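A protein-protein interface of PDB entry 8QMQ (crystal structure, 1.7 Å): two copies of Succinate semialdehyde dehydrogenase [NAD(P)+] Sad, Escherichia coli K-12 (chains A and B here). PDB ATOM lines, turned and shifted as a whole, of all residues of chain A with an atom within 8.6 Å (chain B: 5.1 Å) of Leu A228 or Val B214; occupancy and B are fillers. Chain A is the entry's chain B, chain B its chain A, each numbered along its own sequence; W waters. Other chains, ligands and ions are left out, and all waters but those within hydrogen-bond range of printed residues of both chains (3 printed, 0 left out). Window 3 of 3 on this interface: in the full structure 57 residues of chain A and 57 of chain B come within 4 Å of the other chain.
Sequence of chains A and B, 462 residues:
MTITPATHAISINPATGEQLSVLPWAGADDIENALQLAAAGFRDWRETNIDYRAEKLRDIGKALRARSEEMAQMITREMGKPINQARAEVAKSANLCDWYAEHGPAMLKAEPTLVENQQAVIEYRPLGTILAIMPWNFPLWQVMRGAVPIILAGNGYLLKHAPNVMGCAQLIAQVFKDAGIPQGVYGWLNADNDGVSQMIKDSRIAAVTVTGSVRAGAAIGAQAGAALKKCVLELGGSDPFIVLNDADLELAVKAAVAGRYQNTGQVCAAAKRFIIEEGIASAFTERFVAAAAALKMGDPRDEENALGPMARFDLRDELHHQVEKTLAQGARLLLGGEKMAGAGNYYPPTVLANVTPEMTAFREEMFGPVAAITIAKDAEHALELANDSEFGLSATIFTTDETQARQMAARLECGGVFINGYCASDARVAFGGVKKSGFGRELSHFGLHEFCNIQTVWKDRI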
ATOM      1  N   ILE A 200      18.127  16.497 -18.015  1.00  0.00           N
ATOM      2  CA  ILE A 200      19.504  16.946 -18.229  1.00  0.00           C
ATOM      3  C   ILE A 200      20.246  17.069 -16.900  1.00  0.00           C
ATOM      4  O   ILE A 200      21.439  16.755 -16.811  1.00  0.00           O
ATOM      5  CB  ILE A 200      19.514  18.268 -19.020  1.00  0.00           C
ATOM      6  CG1 ILE A 200      18.956  18.043 -20.431  1.00  0.00           C
ATOM      7  CG2 ILE A 200      20.935  18.833 -19.101  1.00  0.00           C
ATOM      8  CD1 ILE A 200      18.720  19.312 -21.231  1.00  0.00           C
ATOM      9  N   LYS A 201      19.544  17.502 -15.846  1.00  0.00           N
ATOM     10  CA  LYS A 201      20.132  17.660 -14.515  1.00  0.00           C
ATOM     11  C   LYS A 201      20.301  16.342 -13.768  1.00  0.00           C
ATOM     12  O   LYS A 201      21.033  16.296 -12.770  1.00  0.00           O
ATOM     13  CB  LYS A 201      19.267  18.598 -13.663  1.00  0.00           C
ATOM     14  CG  LYS A 201      19.338  20.073 -14.031  1.00  0.00           C
ATOM     15  CD  LYS A 201      18.188  20.839 -13.394  1.00  0.00           C
ATOM     16  CE  LYS A 201      18.375  22.352 -13.508  1.00  0.00           C
ATOM     17  NZ  LYS A 201      17.121  23.081 -13.143  1.00  0.00           N
ATOM     18  N   ILE A 205      21.554  10.694 -16.789  1.00  0.00           N
ATOM     19  CA  ILE A 205      21.768  11.125 -18.164  1.00  0.00           C
ATOM     20  C   ILE A 205      23.221  11.568 -18.281  1.00  0.00           C
ATOM     21  O   ILE A 205      23.655  12.482 -17.567  1.00  0.00           O
ATOM     22  CB  ILE A 205      20.815  12.259 -18.562  1.00  0.00           C
ATOM     23  CG1 ILE A 205      19.361  11.754 -18.569  1.00  0.00           C
ATOM     24  CG2 ILE A 205      21.210  12.840 -19.941  1.00  0.00           C
ATOM     25  CD1 ILE A 205      19.141  10.496 -19.411  1.00  0.00           C
ATOM     26  N   ALA A 206      23.973  10.924 -19.173  1.00  0.00           N
ATOM     27  CA  ALA A 206      25.400  11.201 -19.304  1.00  0.00           C
ATOM     28  C   ALA A 206      25.709  12.330 -20.282  1.00  0.00           C
ATOM     29  O   ALA A 206      26.696  13.044 -20.091  1.00  0.00           O
ATOM     30  CB  ALA A 206      26.146   9.938 -19.743  1.00  0.00           C
ATOM     31  N   ALA A 207      24.904  12.502 -21.328  1.00  0.00           N
ATOM     32  CA  ALA A 207      25.174  13.500 -22.360  1.00  0.00           C
ATOM     33  C   ALA A 207      23.891  13.701 -23.157  1.00  0.00           C
ATOM     34  O   ALA A 207      22.900  13.003 -22.939  1.00  0.00           O
ATOM     35  CB  ALA A 207      26.328  13.073 -23.272  1.00  0.00           C
ATOM     36  N   VAL A 208      23.907  14.683 -24.067  1.00  0.00           N
ATOM     37  CA  VAL A 208      22.697  15.107 -24.774  1.00  0.00           C
ATOM     38  C   VAL A 208      23.007  15.275 -26.257  1.00  0.00           C
ATOM     39  O   VAL A 208      24.068  15.785 -26.626  1.00  0.00           O
ATOM     40  CB  VAL A 208      22.139  16.428 -24.194  1.00  0.00           C
ATOM     41  CG1 VAL A 208      20.764  16.755 -24.799  1.00  0.00           C
ATOM     42  CG2 VAL A 208      22.056  16.378 -22.674  1.00  0.00           C
ATOM     43  N   GLY A 221      21.543  23.493 -25.176  1.00  0.00           N
ATOM     44  CA  GLY A 221      22.986  23.534 -25.017  1.00  0.00           C
ATOM     45  C   GLY A 221      23.407  24.267 -23.758  1.00  0.00           C
ATOM     46  O   GLY A 221      24.353  23.858 -23.077  1.00  0.00           O
ATOM     47  N   ALA A 222      22.709  25.359 -23.425  1.00  0.00           N
ATOM     48  CA  ALA A 222      23.028  26.071 -22.188  1.00  0.00           C
ATOM     49  C   ALA A 222      22.782  25.187 -20.972  1.00  0.00           C
ATOM     50  O   ALA A 222      23.559  25.208 -20.008  1.00  0.00           O
ATOM     51  CB  ALA A 222      22.208  27.359 -22.096  1.00  0.00           C
ATOM     52  N   GLN A 223      21.710  24.390 -21.004  1.00  0.00           N
ATOM     53  CA  GLN A 223      21.410  23.512 -19.875  1.00  0.00           C
ATOM     54  C   GLN A 223      22.411  22.371 -19.780  1.00  0.00           C
ATOM     55  O   GLN A 223      22.829  21.994 -18.675  1.00  0.00           O
ATOM     56  CB  GLN A 223      19.992  22.958 -19.996  1.00  0.00           C
ATOM     57  CG  GLN A 223      18.921  24.007 -19.911  1.00  0.00           C
ATOM     58  CD  GLN A 223      17.548  23.413 -20.133  1.00  0.00           C
ATOM     59  OE1 GLN A 223      17.045  22.677 -19.298  1.00  0.00           O
ATOM     60  NE2 GLN A 223      16.946  23.719 -21.270  1.00  0.00           N
ATOM     61  N   ALA A 224      22.798  21.799 -20.924  1.00  0.00           N
ATOM     62  CA  ALA A 224      23.817  20.752 -20.911  1.00  0.00           C
ATOM     63  C   ALA A 224      25.126  21.277 -20.336  1.00  0.00           C
ATOM     64  O   ALA A 224      25.764  20.621 -19.501  1.00  0.00           O
ATOM     65  CB  ALA A 224      24.033  20.206 -22.323  1.00  0.00           C
ATOM     66  N   GLY A 225      25.544  22.465 -20.775  1.00  0.00           N
ATOM     67  CA  GLY A 225      26.775  23.038 -20.257  1.00  0.00           C
ATOM     68  C   GLY A 225      26.715  23.289 -18.762  1.00  0.00           C
ATOM     69  O   GLY A 225      27.666  22.986 -18.033  1.00  0.00           O
ATOM     70  N   ALA A 226      25.596  23.845 -18.281  1.00  0.00           N
ATOM     71  CA  ALA A 226      25.441  24.092 -16.846  1.00  0.00           C
ATOM     72  C   ALA A 226      25.496  22.805 -16.034  1.00  0.00           C
ATOM     73  O   ALA A 226      25.929  22.820 -14.866  1.00  0.00           O
ATOM     74  CB  ALA A 226      24.124  24.811 -16.577  1.00  0.00           C
ATOM     75  N   ALA A 227      25.039  21.693 -16.609  1.00  0.00           N
ATOM     76  CA  ALA A 227      25.054  20.398 -15.927  1.00  0.00           C
ATOM     77  C   ALA A 227      26.342  19.614 -16.167  1.00  0.00           C
ATOM     78  O   ALA A 227      26.465  18.474 -15.690  1.00  0.00           O
ATOM     79  CB  ALA A 227      23.836  19.571 -16.370  1.00  0.00           C
ATOM     80  N   LEU A 228      27.305  20.205 -16.877  1.00  0.00           N
ATOM     81  CA  LEU A 228      28.568  19.559 -17.248  1.00  0.00           C
ATOM     82  C   LEU A 228      28.326  18.258 -18.012  1.00  0.00           C
ATOM     83  O   LEU A 228      28.973  17.240 -17.769  1.00  0.00           O
ATOM     84  CB  LEU A 228      29.466  19.332 -16.026  1.00  0.00           C
ATOM     85  CG  LEU A 228      29.913  20.637 -15.351  1.00  0.00           C
ATOM     86  CD1 LEU A 228      30.707  20.377 -14.085  1.00  0.00           C
ATOM     87  CD2 LEU A 228      30.716  21.509 -16.314  1.00  0.00           C
ATOM     88  N   LYS A 229      27.384  18.303 -18.953  1.00  0.00           N
ATOM     89  CA  LYS A 229      27.100  17.199 -19.861  1.00  0.00           C
ATOM     90  C   LYS A 229      27.517  17.631 -21.263  1.00  0.00           C
ATOM     91  O   LYS A 229      27.163  18.730 -21.700  1.00  0.00           O
ATOM     92  CB  LYS A 229      25.611  16.841 -19.865  1.00  0.00           C
ATOM     93  CG  LYS A 229      24.934  16.716 -18.492  1.00  0.00           C
ATOM     94  CD  LYS A 229      25.223  15.393 -17.838  1.00  0.00           C
ATOM     95  CE  LYS A 229      24.749  15.355 -16.375  1.00  0.00           C
ATOM     96  NZ  LYS A 229      23.327  14.928 -16.183  1.00  0.00           N
ATOM     97  N   LYS A 230      28.277  16.783 -21.950  1.00  0.00           N
ATOM     98  CA  LYS A 230      28.626  17.045 -23.340  1.00  0.00           C
ATOM     99  C   LYS A 230      27.371  17.051 -24.198  1.00  0.00           C
ATOM    100  O   LYS A 230      26.426  16.301 -23.947  1.00  0.00           O
ATOM    101  CB  LYS A 230      29.590  15.973 -23.853  1.00  0.00           C
ATOM    102  CG  LYS A 230      30.027  16.203 -25.282  1.00  0.00           C
ATOM    103  CD  LYS A 230      30.959  15.120 -25.808  1.00  0.00           C
ATOM    104  CE  LYS A 230      31.078  15.265 -27.332  1.00  0.00           C
ATOM    105  NZ  LYS A 230      32.225  14.518 -27.910  1.00  0.00           N
ATOM    106  N   CYS A 231      27.358  17.901 -25.225  1.00  0.00           N
ATOM    107  CA  CYS A 231      26.264  17.861 -26.182  1.00  0.00           C
ATOM    108  C   CYS A 231      26.798  17.897 -27.607  1.00  0.00           C
ATOM    109  O   CYS A 231      27.927  18.319 -27.870  1.00  0.00           O
ATOM    110  CB  CYS A 231      25.246  19.001 -25.961  1.00  0.00           C
ATOM    111  SG  CYS A 231      25.851  20.687 -26.136  1.00  0.00           S
ATOM    112  N   GLY B 212      40.267  24.339 -15.408  1.00  0.00           N
ATOM    113  CA  GLY B 212      40.021  25.021 -14.149  1.00  0.00           C
ATOM    114  C   GLY B 212      39.125  24.202 -13.239  1.00  0.00           C
ATOM    115  O   GLY B 212      39.013  22.991 -13.393  1.00  0.00           O
ATOM    116  N   SER B 213      38.481  24.896 -12.300  1.00  0.00           N
ATOM    117  CA  SER B 213      37.615  24.246 -11.322  1.00  0.00           C
ATOM    118  C   SER B 213      36.292  23.806 -11.954  1.00  0.00           C
ATOM    119  O   SER B 213      35.886  24.291 -13.015  1.00  0.00           O
ATOM    120  CB  SER B 213      37.314  25.183 -10.156  1.00  0.00           C
ATOM    121  OG  SER B 213      36.502  26.272 -10.570  1.00  0.00           O
ATOM    122  N   VAL B 214      35.614  22.882 -11.263  1.00  0.00           N
ATOM    123  CA  VAL B 214      34.288  22.432 -11.685  1.00  0.00           C
ATOM    124  C   VAL B 214      33.330  23.613 -11.760  1.00  0.00           C
ATOM    125  O   VAL B 214      32.514  23.716 -12.689  1.00  0.00           O
ATOM    126  CB  VAL B 214      33.774  21.335 -10.724  1.00  0.00           C
ATOM    127  CG1 VAL B 214      32.293  21.029 -10.971  1.00  0.00           C
ATOM    128  CG2 VAL B 214      34.612  20.062 -10.856  1.00  0.00           C
ATOM    129  N   ARG B 215      33.428  24.531 -10.792  1.00  0.00           N
ATOM    130  CA  ARG B 215      32.557  25.698 -10.758  1.00  0.00           C
ATOM    131  C   ARG B 215      32.765  26.587 -11.980  1.00  0.00           C
ATOM    132  O   ARG B 215      31.797  27.082 -12.570  1.00  0.00           O
ATOM    133  CB  ARG B 215      32.810  26.489  -9.472  1.00  0.00           C
ATOM    134  CG  ARG B 215      31.985  27.758  -9.349  1.00  0.00           C
ATOM    135  CD  ARG B 215      32.361  28.575  -8.109  1.00  0.00           C
ATOM    136  NE  ARG B 215      31.636  29.842  -8.074  1.00  0.00           N
ATOM    137  CZ  ARG B 215      31.773  30.768  -7.133  1.00  0.00           C
ATOM    138  NH1 ARG B 215      32.604  30.603  -6.114  1.00  0.00           N
ATOM    139  NH2 ARG B 215      31.059  31.888  -7.218  1.00  0.00           N
ATOM    140  N   ALA B 216      34.025  26.814 -12.360  1.00  0.00           N
ATOM    141  CA  ALA B 216      34.308  27.632 -13.536  1.00  0.00           C
ATOM    142  C   ALA B 216      33.819  26.953 -14.804  1.00  0.00           C
ATOM    143  O   ALA B 216      33.255  27.612 -15.689  1.00  0.00           O
ATOM    144  CB  ALA B 216      35.808  27.912 -13.643  1.00  0.00           C
ATOM    145  N   GLY B 217      34.041  25.642 -14.911  1.00  0.00           N
ATOM    146  CA  GLY B 217      33.590  24.910 -16.084  1.00  0.00           C
ATOM    147  C   GLY B 217      32.087  24.969 -16.279  1.00  0.00           C
ATOM    148  O   GLY B 217      31.605  25.104 -17.410  1.00  0.00           O
ATOM    149  N   ALA B 218      31.322  24.859 -15.191  1.00  0.00           N
ATOM    150  CA  ALA B 218      29.867  24.911 -15.337  1.00  0.00           C
ATOM    151  C   ALA B 218      29.399  26.313 -15.713  1.00  0.00           C
ATOM    152  O   ALA B 218      28.486  26.474 -16.534  1.00  0.00           O
ATOM    153  CB  ALA B 218      29.192  24.441 -14.050  1.00  0.00           C
ATOM    154  N   ALA B 219      30.013  27.342 -15.125  1.00  0.00           N
ATOM    155  CA  ALA B 219      29.652  28.715 -15.464  1.00  0.00           C
ATOM    156  C   ALA B 219      29.978  29.029 -16.918  1.00  0.00           C
ATOM    157  O   ALA B 219      29.171  29.639 -17.632  1.00  0.00           O
ATOM    158  CB  ALA B 219      30.377  29.688 -14.530  1.00  0.00           C
ATOM    159  N   LEU B 233      36.078  21.060 -21.719  1.00  0.00           N
ATOM    160  CA  LEU B 233      36.175  21.370 -20.296  1.00  0.00           C
ATOM    161  C   LEU B 233      37.073  20.344 -19.627  1.00  0.00           C
ATOM    162  O   LEU B 233      36.757  19.150 -19.619  1.00  0.00           O
ATOM    163  CB  LEU B 233      34.798  21.372 -19.628  1.00  0.00           C
ATOM    164  CG  LEU B 233      33.753  22.322 -20.216  1.00  0.00           C
ATOM    165  CD1 LEU B 233      32.498  22.263 -19.368  1.00  0.00           C
ATOM    166  CD2 LEU B 233      34.296  23.746 -20.307  1.00  0.00           C
ATOM    167  N   LEU B 235      38.427  19.815 -16.024  1.00  0.00           N
ATOM    168  CA  LEU B 235      38.110  20.398 -14.749  1.00  0.00           C
ATOM    169  C   LEU B 235      38.849  19.606 -13.670  1.00  0.00           C
ATOM    170  O   LEU B 235      39.874  18.965 -13.951  1.00  0.00           O
ATOM    171  CB  LEU B 235      36.582  20.458 -14.580  1.00  0.00           C
ATOM    172  CG  LEU B 235      35.884  21.062 -15.817  1.00  0.00           C
ATOM    173  CD1 LEU B 235      34.362  21.094 -15.655  1.00  0.00           C
ATOM    174  CD2 LEU B 235      36.420  22.460 -16.097  1.00  0.00           C
ATOM    175  N   GLY B 236      38.351  19.648 -12.447  1.00  0.00           N
ATOM    176  CA  GLY B 236      39.110  19.028 -11.376  1.00  0.00           C
ATOM    177  C   GLY B 236      39.271  17.515 -11.531  1.00  0.00           C
ATOM    178  O   GLY B 236      38.756  16.869 -12.447  1.00  0.00           O
ATOM    179  N   PHE B 391      34.003  13.271  -9.571  1.00  0.00           N
ATOM    180  CA  PHE B 391      35.110  13.467 -10.495  1.00  0.00           C
ATOM    181  C   PHE B 391      35.385  12.196 -11.290  1.00  0.00           C
ATOM    182  O   PHE B 391      34.968  11.093 -10.922  1.00  0.00           O
ATOM    183  CB  PHE B 391      36.383  13.878  -9.743  1.00  0.00           C
ATOM    184  CG  PHE B 391      36.258  15.183  -8.998  1.00  0.00           C
ATOM    185  CD1 PHE B 391      36.514  16.390  -9.635  1.00  0.00           C
ATOM    186  CD2 PHE B 391      35.877  15.203  -7.667  1.00  0.00           C
ATOM    187  CE1 PHE B 391      36.398  17.589  -8.952  1.00  0.00           C
ATOM    188  CE2 PHE B 391      35.757  16.397  -6.979  1.00  0.00           C
ATOM    189  CZ  PHE B 391      36.019  17.590  -7.625  1.00  0.00           C
ATOM    190  N   LYS B 435      32.249  12.754 -16.266  1.00  0.00           N
ATOM    191  CA  LYS B 435      31.477  13.218 -15.090  1.00  0.00           C
ATOM    192  C   LYS B 435      31.828  14.694 -14.845  1.00  0.00           C
ATOM    193  O   LYS B 435      31.935  15.472 -15.812  1.00  0.00           O
ATOM    194  CB  LYS B 435      31.725  12.258 -13.912  1.00  0.00           C
ATOM    195  CG  LYS B 435      31.132  10.865 -14.183  1.00  0.00           C
ATOM    196  CD  LYS B 435      31.762   9.755 -13.324  1.00  0.00           C
ATOM    197  CE  LYS B 435      31.469   9.943 -11.866  1.00  0.00           C
ATOM    198  NZ  LYS B 435      31.919   8.756 -11.061  1.00  0.00           N
ATOM    199  N   LYS B 436      31.997  15.129 -13.593  1.00  0.00           N
ATOM    200  CA  LYS B 436      32.261  16.548 -13.358  1.00  0.00           C
ATOM    201  C   LYS B 436      33.699  16.953 -13.676  1.00  0.00           C
ATOM    202  O   LYS B 436      34.011  18.150 -13.630  1.00  0.00           O
ATOM    203  CB  LYS B 436      31.891  16.928 -11.916  1.00  0.00           C
ATOM    204  CG  LYS B 436      30.381  16.792 -11.623  1.00  0.00           C
ATOM    205  CD  LYS B 436      29.891  17.825 -10.624  1.00  0.00           C
ATOM    206  CE  LYS B 436      28.446  17.568 -10.201  1.00  0.00           C
ATOM    207  NZ  LYS B 436      27.572  17.291 -11.362  1.00  0.00           N
ATOM    208  N   PHE B 439      34.573  17.103 -20.292  1.00  0.00           N
ATOM    209  CA  PHE B 439      34.430  16.345 -21.533  1.00  0.00           C
ATOM    210  C   PHE B 439      35.354  16.961 -22.580  1.00  0.00           C
ATOM    211  O   PHE B 439      35.875  18.067 -22.408  1.00  0.00           O
ATOM    212  CB  PHE B 439      32.972  16.322 -22.022  1.00  0.00           C
ATOM    213  CG  PHE B 439      32.304  17.661 -21.982  1.00  0.00           C
ATOM    214  CD1 PHE B 439      32.563  18.615 -22.955  1.00  0.00           C
ATOM    215  CD2 PHE B 439      31.409  17.963 -20.966  1.00  0.00           C
ATOM    216  CE1 PHE B 439      31.952  19.849 -22.906  1.00  0.00           C
ATOM    217  CE2 PHE B 439      30.788  19.192 -20.912  1.00  0.00           C
ATOM    218  CZ  PHE B 439      31.063  20.140 -21.887  1.00  0.00           C
HETATM  219  O   HOH W   1      25.216  17.537 -13.405  1.00  0.00           O
HETATM  220  O   HOH W   2      28.545  14.937 -15.889  1.00  0.00           O
HETATM  221  O   HOH W   3      30.785  15.267 -18.309  1.00  0.00           O
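No position is printed for both chains.
Lys A201 touches none of the printed residues of chain B. Val B214 touches just one residue of chain A: Leu A228. Of chain A, only Leu A228 comes within 4 Å of Gly B217. Ala B219 touches none of the printed residues of chain A. Of the printed residues of chain A, Leu B233 touches Leu A228. Of the printed residues of chain A, Lys B435 touches Leu A228. The nearest printed residue of chain B that does not touch Leu A228 is Lys B436 (4.01 Å). The nearest residue of chain A that does not touch Val B214 is Ala A226 (7.0 Å).
Hydrophobic or aromatic side chains of chain A within 4 Å of the printed part of chain B: Leu A228. Among the printed residues, no Asp or Glu carboxylate lies within 4 Å of a Lys or Arg side-chain nitrogen of the other chain.
O of Gly A225 touches O of Ala B218 (3.9 Å). O of Ala A226 touches CB of Ala B218 (3.7 Å). CD1 of Leu A228 touches CG1 of Val B214, at 3.6 Å. Leu A228 touches Gly B217. CD2 of Leu A228 touches CD1 of Leu B233, 3.6 Å away. CD1 of Leu B235 touches CD2 of Leu A228, at 3.7 Å. Leu A228 touches Lys B435 (O to O, 3.97 Å). C of Leu A228 touches CE2 of Phe B439 (3.9 Å). Lys A229 touches Phe B439. Lys A230 touches Phe B439.
Water W3 lies within hydrogen-bond range of O of Leu A228 (2.7 Å) and O of Lys B435 (2.8 Å). Water W1 lies within hydrogen-bond range of O of Ala A227 and NZ of Lys B436. Water W2 lies within hydrogen-bond range of O of Leu A228 (3.0 Å) and O of Lys B435 (3.4 Å).
The backbone carbonyl oxygen of Leu B233 is in hydrogen-bond range of the backbone NH of Phe B439, 3.1 Å away. The backbone carbonyl oxygen (O) of Ile A200 sits at hydrogen-bond distance from the side-chain amino group (NZ) of Lys A229 (2.7 Å). The backbone carbonyl oxygen (O) of Ile A205 lies within hydrogen-bond range of the side-chain amino group (NZ) of Lys A229 (2.8 Å). O of Lys A230 is in hydrogen-bond range of N of Val A208. The backbone NH of Lys A229 is in hydrogen-bond range of the backbone carbonyl oxygen of Ala A224 (2.9 Å).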
